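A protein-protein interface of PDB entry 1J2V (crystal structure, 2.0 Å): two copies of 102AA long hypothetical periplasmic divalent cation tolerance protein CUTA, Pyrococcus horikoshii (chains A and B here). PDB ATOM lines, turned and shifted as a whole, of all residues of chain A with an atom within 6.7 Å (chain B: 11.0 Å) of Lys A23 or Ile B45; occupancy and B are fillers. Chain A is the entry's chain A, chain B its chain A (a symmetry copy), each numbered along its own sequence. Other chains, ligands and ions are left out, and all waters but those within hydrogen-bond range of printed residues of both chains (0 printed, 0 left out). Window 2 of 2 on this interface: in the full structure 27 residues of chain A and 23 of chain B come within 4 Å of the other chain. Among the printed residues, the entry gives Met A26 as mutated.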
ATOM      1  N   GLU A  15       6.303   5.970 -11.984  1.00  0.00           N
ATOM      2  CA  GLU A  15       5.398   7.100 -11.834  1.00  0.00           C
ATOM      3  C   GLU A  15       6.090   8.158 -10.974  1.00  0.00           C
ATOM      4  O   GLU A  15       6.016   9.354 -11.267  1.00  0.00           O
ATOM      5  CB  GLU A  15       4.120   6.627 -11.165  1.00  0.00           C
ATOM      6  CG  GLU A  15       3.539   5.433 -11.861  1.00  0.00           C
ATOM      7  CD  GLU A  15       2.259   4.939 -11.232  1.00  0.00           C
ATOM      8  OE1 GLU A  15       2.113   5.041  -9.992  1.00  0.00           O
ATOM      9  OE2 GLU A  15       1.416   4.414 -11.985  1.00  0.00           O
ATOM     10  N   LYS A  16       6.768   7.715  -9.921  1.00  0.00           N
ATOM     11  CA  LYS A  16       7.462   8.637  -9.040  1.00  0.00           C
ATOM     12  C   LYS A  16       8.515   9.415  -9.842  1.00  0.00           C
ATOM     13  O   LYS A  16       8.510  10.647  -9.846  1.00  0.00           O
ATOM     14  CB  LYS A  16       8.124   7.861  -7.905  1.00  0.00           C
ATOM     15  CG  LYS A  16       8.434   8.686  -6.670  1.00  0.00           C
ATOM     16  CD  LYS A  16       8.037  10.153  -6.815  1.00  0.00           C
ATOM     17  CE  LYS A  16       6.886  10.550  -5.884  1.00  0.00           C
ATOM     18  NZ  LYS A  16       6.674  12.030  -5.896  1.00  0.00           N
ATOM     19  N   VAL A  18       8.899   9.662 -13.132  1.00  0.00           N
ATOM     20  CA  VAL A  18       8.262  10.382 -14.238  1.00  0.00           C
ATOM     21  C   VAL A  18       7.511  11.654 -13.835  1.00  0.00           C
ATOM     22  O   VAL A  18       7.612  12.669 -14.525  1.00  0.00           O
ATOM     23  CB  VAL A  18       7.287   9.461 -15.037  1.00  0.00           C
ATOM     24  CG1 VAL A  18       6.406  10.296 -15.964  1.00  0.00           C
ATOM     25  CG2 VAL A  18       8.068   8.500 -15.911  1.00  0.00           C
ATOM     26  N   LYS A  19       6.744  11.607 -12.745  1.00  0.00           N
ATOM     27  CA  LYS A  19       6.004  12.796 -12.324  1.00  0.00           C
ATOM     28  C   LYS A  19       6.972  13.828 -11.767  1.00  0.00           C
ATOM     29  O   LYS A  19       6.798  15.030 -11.951  1.00  0.00           O
ATOM     30  CB  LYS A  19       4.889  12.432 -11.319  1.00  0.00           C
ATOM     31  CG  LYS A  19       3.518  12.196 -12.009  1.00  0.00           C
ATOM     32  CD  LYS A  19       2.390  11.799 -11.056  1.00  0.00           C
ATOM     33  CE  LYS A  19       2.542  10.352 -10.570  1.00  0.00           C
ATOM     34  NZ  LYS A  19       1.477   9.937  -9.608  1.00  0.00           N
ATOM     35  N   THR A  20       8.017  13.351 -11.111  1.00  0.00           N
ATOM     36  CA  THR A  20       9.024  14.254 -10.586  1.00  0.00           C
ATOM     37  C   THR A  20       9.609  15.007 -11.785  1.00  0.00           C
ATOM     38  O   THR A  20       9.726  16.237 -11.760  1.00  0.00           O
ATOM     39  CB  THR A  20      10.148  13.471  -9.854  1.00  0.00           C
ATOM     40  OG1 THR A  20       9.674  13.042  -8.568  1.00  0.00           O
ATOM     41  CG2 THR A  20      11.394  14.333  -9.675  1.00  0.00           C
ATOM     42  N   LEU A  21       9.953  14.262 -12.837  1.00  0.00           N
ATOM     43  CA  LEU A  21      10.538  14.854 -14.039  1.00  0.00           C
ATOM     44  C   LEU A  21       9.634  15.890 -14.714  1.00  0.00           C
ATOM     45  O   LEU A  21      10.115  16.940 -15.141  1.00  0.00           O
ATOM     46  CB  LEU A  21      10.928  13.759 -15.038  1.00  0.00           C
ATOM     47  CG  LEU A  21      11.965  12.755 -14.531  1.00  0.00           C
ATOM     48  CD1 LEU A  21      12.305  11.761 -15.640  1.00  0.00           C
ATOM     49  CD2 LEU A  21      13.221  13.496 -14.056  1.00  0.00           C
ATOM     50  N   LEU A  22       8.338  15.595 -14.819  1.00  0.00           N
ATOM     51  CA  LEU A  22       7.381  16.522 -15.420  1.00  0.00           C
ATOM     52  C   LEU A  22       7.277  17.767 -14.540  1.00  0.00           C
ATOM     53  O   LEU A  22       7.333  18.894 -15.034  1.00  0.00           O
ATOM     54  CB  LEU A  22       5.994  15.875 -15.547  1.00  0.00           C
ATOM     55  CG  LEU A  22       5.650  15.017 -16.771  1.00  0.00           C
ATOM     56  CD1 LEU A  22       4.332  14.289 -16.548  1.00  0.00           C
ATOM     57  CD2 LEU A  22       5.562  15.895 -17.983  1.00  0.00           C
ATOM     58  N   LYS A  23       7.126  17.560 -13.231  1.00  0.00           N
ATOM     59  CA  LYS A  23       7.029  18.685 -12.297  1.00  0.00           C
ATOM     60  C   LYS A  23       8.196  19.608 -12.576  1.00  0.00           C
ATOM     61  O   LYS A  23       8.004  20.763 -12.963  1.00  0.00           O
ATOM     62  CB  LYS A  23       7.079  18.204 -10.841  1.00  0.00           C
ATOM     63  CG  LYS A  23       5.942  17.258 -10.464  1.00  0.00           C
ATOM     64  CD  LYS A  23       5.481  17.432  -9.030  1.00  0.00           C
ATOM     65  CE  LYS A  23       4.579  16.282  -8.606  1.00  0.00           C
ATOM     66  NZ  LYS A  23       5.342  14.996  -8.601  1.00  0.00           N
ATOM     67  N   GLU A  24       9.406  19.074 -12.403  1.00  0.00           N
ATOM     68  CA  GLU A  24      10.637  19.813 -12.651  1.00  0.00           C
ATOM     69  C   GLU A  24      10.674  20.320 -14.101  1.00  0.00           C
ATOM     70  O   GLU A  24      11.519  21.123 -14.451  1.00  0.00           O
ATOM     71  CB  GLU A  24      11.852  18.912 -12.364  1.00  0.00           C
ATOM     72  CG  GLU A  24      11.945  18.438 -10.908  1.00  0.00           C
ATOM     73  CD  GLU A  24      13.148  17.546 -10.628  1.00  0.00           C
ATOM     74  OE1 GLU A  24      13.384  17.207  -9.447  1.00  0.00           O
ATOM     75  OE2 GLU A  24      13.864  17.172 -11.578  1.00  0.00           O
ATOM     76  N   ARG A  25       9.742  19.848 -14.928  1.00  0.00           N
ATOM     77  CA  ARG A  25       9.613  20.226 -16.347  1.00  0.00           C
ATOM     78  C   ARG A  25      10.776  19.822 -17.259  1.00  0.00           C
ATOM     79  O   ARG A  25      11.057  20.450 -18.295  1.00  0.00           O
ATOM     80  CB  ARG A  25       9.328  21.723 -16.459  1.00  0.00           C
ATOM     81  CG  ARG A  25       7.888  22.043 -16.071  1.00  0.00           C
ATOM     82  CD  ARG A  25       7.539  23.512 -16.197  1.00  0.00           C
ATOM     83  NE  ARG A  25       6.111  23.717 -15.970  1.00  0.00           N
ATOM     84  CZ  ARG A  25       5.157  23.329 -16.813  1.00  0.00           C
ATOM     85  NH1 ARG A  25       5.488  22.717 -17.947  1.00  0.00           N
ATOM     86  NH2 ARG A  25       3.873  23.553 -16.521  1.00  0.00           N
ATOM     87  N   MET A  26      11.425  18.732 -16.871  1.00  0.00           N
ATOM     88  CA  MET A  26      12.561  18.166 -17.592  1.00  0.00           C
ATOM     89  C   MET A  26      12.097  17.490 -18.885  1.00  0.00           C
ATOM     90  O   MET A  26      12.878  17.302 -19.826  1.00  0.00           O
ATOM     91  CB  MET A  26      13.237  17.132 -16.689  1.00  0.00           C
ATOM     92  CG  MET A  26      13.843  17.729 -15.447  1.00  0.00           C
ATOM     93  SD  MET A  26      15.399  18.454 -15.916  1.00  0.00           S
ATOM     94  CE  MET A  26      16.432  17.176 -15.496  1.00  0.00           C
ATOM     95  N   ILE A  27      10.824  17.109 -18.897  1.00  0.00           N
ATOM     96  CA  ILE A  27      10.219  16.444 -20.030  1.00  0.00           C
ATOM     97  C   ILE A  27       8.814  16.948 -20.113  1.00  0.00           C
ATOM     98  O   ILE A  27       8.250  17.386 -19.108  1.00  0.00           O
ATOM     99  CB  ILE A  27      10.144  14.904 -19.842  1.00  0.00           C
ATOM    100  CG1 ILE A  27       9.192  14.562 -18.691  1.00  0.00           C
ATOM    101  CG2 ILE A  27      11.537  14.343 -19.584  1.00  0.00           C
ATOM    102  CD1 ILE A  27       8.815  13.122 -18.573  1.00  0.00           C
ATOM    103  N   ARG B  36       0.216   3.998 -20.349  1.00  0.00           N
ATOM    104  CA  ARG B  36      -0.348   5.042 -19.491  1.00  0.00           C
ATOM    105  C   ARG B  36       0.395   6.358 -19.747  1.00  0.00           C
ATOM    106  O   ARG B  36       1.616   6.445 -19.576  1.00  0.00           O
ATOM    107  CB  ARG B  36      -0.203   4.649 -18.025  1.00  0.00           C
ATOM    108  CG  ARG B  36      -0.474   3.178 -17.725  1.00  0.00           C
ATOM    109  CD  ARG B  36      -1.736   2.909 -16.916  1.00  0.00           C
ATOM    110  NE  ARG B  36      -2.899   2.665 -17.767  1.00  0.00           N
ATOM    111  CZ  ARG B  36      -3.974   1.971 -17.389  1.00  0.00           C
ATOM    112  NH1 ARG B  36      -4.042   1.451 -16.184  1.00  0.00           N
ATOM    113  NH2 ARG B  36      -4.996   1.775 -18.207  1.00  0.00           N
ATOM    114  N   ALA B  37      -0.343   7.360 -20.207  1.00  0.00           N
ATOM    115  CA  ALA B  37       0.228   8.679 -20.481  1.00  0.00           C
ATOM    116  C   ALA B  37       0.275   9.589 -19.250  1.00  0.00           C
ATOM    117  O   ALA B  37      -0.697   9.711 -18.519  1.00  0.00           O
ATOM    118  CB  ALA B  37      -0.562   9.371 -21.580  1.00  0.00           C
ATOM    119  N   PHE B  38       1.422  10.209 -19.019  1.00  0.00           N
ATOM    120  CA  PHE B  38       1.594  11.135 -17.909  1.00  0.00           C
ATOM    121  C   PHE B  38       2.037  12.391 -18.607  1.00  0.00           C
ATOM    122  O   PHE B  38       3.166  12.452 -19.085  1.00  0.00           O
ATOM    123  CB  PHE B  38       2.723  10.710 -16.967  1.00  0.00           C
ATOM    124  CG  PHE B  38       2.480   9.418 -16.255  1.00  0.00           C
ATOM    125  CD1 PHE B  38       2.598   8.197 -16.927  1.00  0.00           C
ATOM    126  CD2 PHE B  38       2.127   9.418 -14.908  1.00  0.00           C
ATOM    127  CE1 PHE B  38       2.370   7.008 -16.274  1.00  0.00           C
ATOM    128  CE2 PHE B  38       1.897   8.224 -14.244  1.00  0.00           C
ATOM    129  CZ  PHE B  38       2.017   7.017 -14.929  1.00  0.00           C
ATOM    130  N   TYR B  39       1.174  13.392 -18.695  1.00  0.00           N
ATOM    131  CA  TYR B  39       1.609  14.590 -19.379  1.00  0.00           C
ATOM    132  C   TYR B  39       1.057  15.916 -18.878  1.00  0.00           C
ATOM    133  O   TYR B  39       0.037  15.981 -18.184  1.00  0.00           O
ATOM    134  CB  TYR B  39       1.322  14.483 -20.872  1.00  0.00           C
ATOM    135  CG  TYR B  39      -0.145  14.327 -21.193  1.00  0.00           C
ATOM    136  CD1 TYR B  39      -0.806  13.122 -20.944  1.00  0.00           C
ATOM    137  CD2 TYR B  39      -0.893  15.401 -21.675  1.00  0.00           C
ATOM    138  CE1 TYR B  39      -2.174  12.992 -21.164  1.00  0.00           C
ATOM    139  CE2 TYR B  39      -2.268  15.281 -21.888  1.00  0.00           C
ATOM    140  CZ  TYR B  39      -2.895  14.076 -21.629  1.00  0.00           C
ATOM    141  OH  TYR B  39      -4.242  13.947 -21.826  1.00  0.00           O
ATOM    142  N   TRP B  40       1.767  16.977 -19.228  1.00  0.00           N
ATOM    143  CA  TRP B  40       1.371  18.317 -18.850  1.00  0.00           C
ATOM    144  C   TRP B  40       0.218  18.712 -19.745  1.00  0.00           C
ATOM    145  O   TRP B  40       0.326  18.730 -20.975  1.00  0.00           O
ATOM    146  CB  TRP B  40       2.535  19.291 -19.051  1.00  0.00           C
ATOM    147  CG  TRP B  40       3.342  19.536 -17.813  1.00  0.00           C
ATOM    148  CD1 TRP B  40       4.665  19.238 -17.619  1.00  0.00           C
ATOM    149  CD2 TRP B  40       2.873  20.098 -16.581  1.00  0.00           C
ATOM    150  NE1 TRP B  40       5.048  19.574 -16.337  1.00  0.00           N
ATOM    151  CE2 TRP B  40       3.970  20.102 -15.678  1.00  0.00           C
ATOM    152  CE3 TRP B  40       1.631  20.591 -16.149  1.00  0.00           C
ATOM    153  CZ2 TRP B  40       3.861  20.588 -14.371  1.00  0.00           C
ATOM    154  CZ3 TRP B  40       1.520  21.070 -14.851  1.00  0.00           C
ATOM    155  CH2 TRP B  40       2.633  21.062 -13.973  1.00  0.00           C
ATOM    156  N   TRP B  41      -0.915  18.972 -19.117  1.00  0.00           N
ATOM    157  CA  TRP B  41      -2.101  19.394 -19.838  1.00  0.00           C
ATOM    158  C   TRP B  41      -2.737  20.561 -19.102  1.00  0.00           C
ATOM    159  O   TRP B  41      -2.965  20.535 -17.877  1.00  0.00           O
ATOM    160  CB  TRP B  41      -3.110  18.281 -19.949  1.00  0.00           C
ATOM    161  CG  TRP B  41      -4.122  18.538 -21.040  1.00  0.00           C
ATOM    162  CD1 TRP B  41      -5.478  18.719 -20.890  1.00  0.00           C
ATOM    163  CD2 TRP B  41      -3.851  18.714 -22.441  1.00  0.00           C
ATOM    164  NE1 TRP B  41      -6.057  18.995 -22.112  1.00  0.00           N
ATOM    165  CE2 TRP B  41      -5.083  18.988 -23.076  1.00  0.00           C
ATOM    166  CE3 TRP B  41      -2.688  18.650 -23.219  1.00  0.00           C
ATOM    167  CZ2 TRP B  41      -5.178  19.215 -24.454  1.00  0.00           C
ATOM    168  CZ3 TRP B  41      -2.786  18.873 -24.573  1.00  0.00           C
ATOM    169  CH2 TRP B  41      -4.021  19.146 -25.183  1.00  0.00           C
ATOM    170  N   GLU B  42      -2.950  21.606 -19.882  1.00  0.00           N
ATOM    171  CA  GLU B  42      -3.524  22.856 -19.411  1.00  0.00           C
ATOM    172  C   GLU B  42      -3.308  23.150 -17.903  1.00  0.00           C
ATOM    173  O   GLU B  42      -2.234  23.609 -17.547  1.00  0.00           O
ATOM    174  CB  GLU B  42      -4.964  22.835 -19.809  1.00  0.00           C
ATOM    175  CG  GLU B  42      -5.200  22.554 -21.306  1.00  0.00           C
ATOM    176  CD  GLU B  42      -6.662  22.419 -21.704  1.00  0.00           C
ATOM    177  OE1 GLU B  42      -6.919  22.399 -22.925  1.00  0.00           O
ATOM    178  OE2 GLU B  42      -7.541  22.334 -20.824  1.00  0.00           O
ATOM    179  N   GLY B  43      -4.242  22.823 -17.017  1.00  0.00           N
ATOM    180  CA  GLY B  43      -3.970  23.114 -15.621  1.00  0.00           C
ATOM    181  C   GLY B  43      -3.474  22.029 -14.697  1.00  0.00           C
ATOM    182  O   GLY B  43      -3.540  22.225 -13.489  1.00  0.00           O
ATOM    183  N   LYS B  44      -2.952  20.918 -15.217  1.00  0.00           N
ATOM    184  CA  LYS B  44      -2.530  19.840 -14.311  1.00  0.00           C
ATOM    185  C   LYS B  44      -1.708  18.704 -14.935  1.00  0.00           C
ATOM    186  O   LYS B  44      -1.644  18.594 -16.144  1.00  0.00           O
ATOM    187  CB  LYS B  44      -3.774  19.237 -13.635  1.00  0.00           C
ATOM    188  CG  LYS B  44      -4.993  19.026 -14.597  1.00  0.00           C
ATOM    189  CD  LYS B  44      -6.164  18.301 -13.917  1.00  0.00           C
ATOM    190  CE  LYS B  44      -7.407  18.222 -14.810  1.00  0.00           C
ATOM    191  NZ  LYS B  44      -8.045  16.870 -14.788  1.00  0.00           N
ATOM    192  N   ILE B  45      -1.011  17.894 -14.131  1.00  0.00           N
ATOM    193  CA  ILE B  45      -0.286  16.779 -14.725  1.00  0.00           C
ATOM    194  C   ILE B  45      -1.366  15.695 -14.837  1.00  0.00           C
ATOM    195  O   ILE B  45      -1.823  15.145 -13.815  1.00  0.00           O
ATOM    196  CB  ILE B  45       0.852  16.185 -13.839  1.00  0.00           C
ATOM    197  CG1 ILE B  45       2.140  16.999 -13.993  1.00  0.00           C
ATOM    198  CG2 ILE B  45       1.164  14.712 -14.353  1.00  0.00           C
ATOM    199  CD1 ILE B  45       3.060  16.891 -12.799  1.00  0.00           C
ATOM    200  N   GLU B  46      -1.817  15.411 -16.048  1.00  0.00           N
ATOM    201  CA  GLU B  46      -2.809  14.367 -16.199  1.00  0.00           C
ATOM    202  C   GLU B  46      -2.209  12.986 -16.374  1.00  0.00           C
ATOM    203  O   GLU B  46      -1.030  12.826 -16.727  1.00  0.00           O
ATOM    204  CB  GLU B  46      -3.745  14.672 -17.369  1.00  0.00           C
ATOM    205  CG  GLU B  46      -5.120  15.224 -16.946  1.00  0.00           C
ATOM    206  CD  GLU B  46      -6.242  14.156 -16.980  1.00  0.00           C
ATOM    207  OE1 GLU B  46      -6.754  13.765 -15.905  1.00  0.00           O
ATOM    208  OE2 GLU B  46      -6.613  13.715 -18.090  1.00  0.00           O
ATOM    209  N   GLU B  47      -3.052  11.995 -16.110  1.00  0.00           N
ATOM    210  CA  GLU B  47      -2.701  10.601 -16.231  1.00  0.00           C
ATOM    211  C   GLU B  47      -3.924   9.908 -16.797  1.00  0.00           C
ATOM    212  O   GLU B  47      -4.981   9.933 -16.178  1.00  0.00           O
ATOM    213  CB  GLU B  47      -2.414   9.999 -14.862  1.00  0.00           C
ATOM    214  CG  GLU B  47      -1.002  10.161 -14.339  1.00  0.00           C
ATOM    215  CD  GLU B  47      -0.794   9.427 -13.014  1.00  0.00           C
ATOM    216  OE1 GLU B  47      -0.954   8.182 -12.989  1.00  0.00           O
ATOM    217  OE2 GLU B  47      -0.479  10.094 -11.998  1.00  0.00           O
ATOM    218  N   ASP B  48      -3.788   9.296 -17.967  1.00  0.00           N
ATOM    219  CA  ASP B  48      -4.892   8.560 -18.559  1.00  0.00           C
ATOM    220  C   ASP B  48      -4.355   7.337 -19.276  1.00  0.00           C
ATOM    221  O   ASP B  48      -3.157   7.065 -19.243  1.00  0.00           O
ATOM    222  CB  ASP B  48      -5.700   9.444 -19.527  1.00  0.00           C
ATOM    223  CG  ASP B  48      -4.878   9.947 -20.721  1.00  0.00           C
ATOM    224  OD1 ASP B  48      -5.452  10.659 -21.580  1.00  0.00           O
ATOM    225  OD2 ASP B  48      -3.671   9.638 -20.804  1.00  0.00           O
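The backbone carbonyl oxygen (O) of Leu A22 is in hydrogen-bond range of the indole nitrogen (NE1) of Trp B40 (2.7 Å). NZ of Lys A19 is in salt-bridge range of OE2 of Glu B47.
The backbone carbonyl oxygen (O) of Tyr B39 sits at hydrogen-bond distance from the backbone NH (N) of Glu B46 (2.9 Å).
Among the printed residues, merely in contact across the chains: Leu A22 with Phe B38 (3.3 Å), Arg A25 with Trp B40 (3.6 Å), Lys A23 with Ile B45 (3.7 Å), Glu A15 with Phe B38 (3.8 Å), Val A18 with Phe B38 (3.8 Å), Leu A22 with Ile B45 (3.9 Å) and Leu A22 with Tyr B39 (3.9 Å).
Of the printed residues of chain B, Glu A15 touches Phe B38. Of the printed residues of chain B, Val A18 touches Phe B38. Of chain B, only Glu B47 comes within 4 Å of Lys A19. No residue of chain B comes within 4 Å of Thr A20. Of the printed residues of chain B, Leu A22 touches Phe B38, Tyr B39, Trp B40 and Ile B45. Lys A23 touches one residue of chain B. No residue of chain B comes within 4 Å of Glu A24. Arg A25 touches one residue of chain B. Ala B37 touches none of the printed residues of chain A. Printed residues of chain A within 4 Å of Phe B38: Glu A15, Val A18 and Leu A22. Printed residues of chain A within 4 Å of Trp B40: Leu A22 and Arg A25. Gly B43 touches none of the printed residues of chain A. Ile B45 touches just these residues of chain A: Leu A22 and Lys A23. Of the printed residues of chain A, Glu B47 touches Lys A19 (3.1 Å).
Printed residues of chain A that touch a printed residue of chain B: Glu A15, Val A18, Lys A19, Leu A22, Lys A23 and Arg A25. Hydrophobic or aromatic side chains of chain A that line the printed part of chain B: Val A18 and Leu A22. Hydrophobic or aromatic side chains of chain B that line the printed part of chain A: Phe B38, Trp B40 and Ile B45. Among the printed residues, 9 pairs touch across the chains.
No position is printed for both chains.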
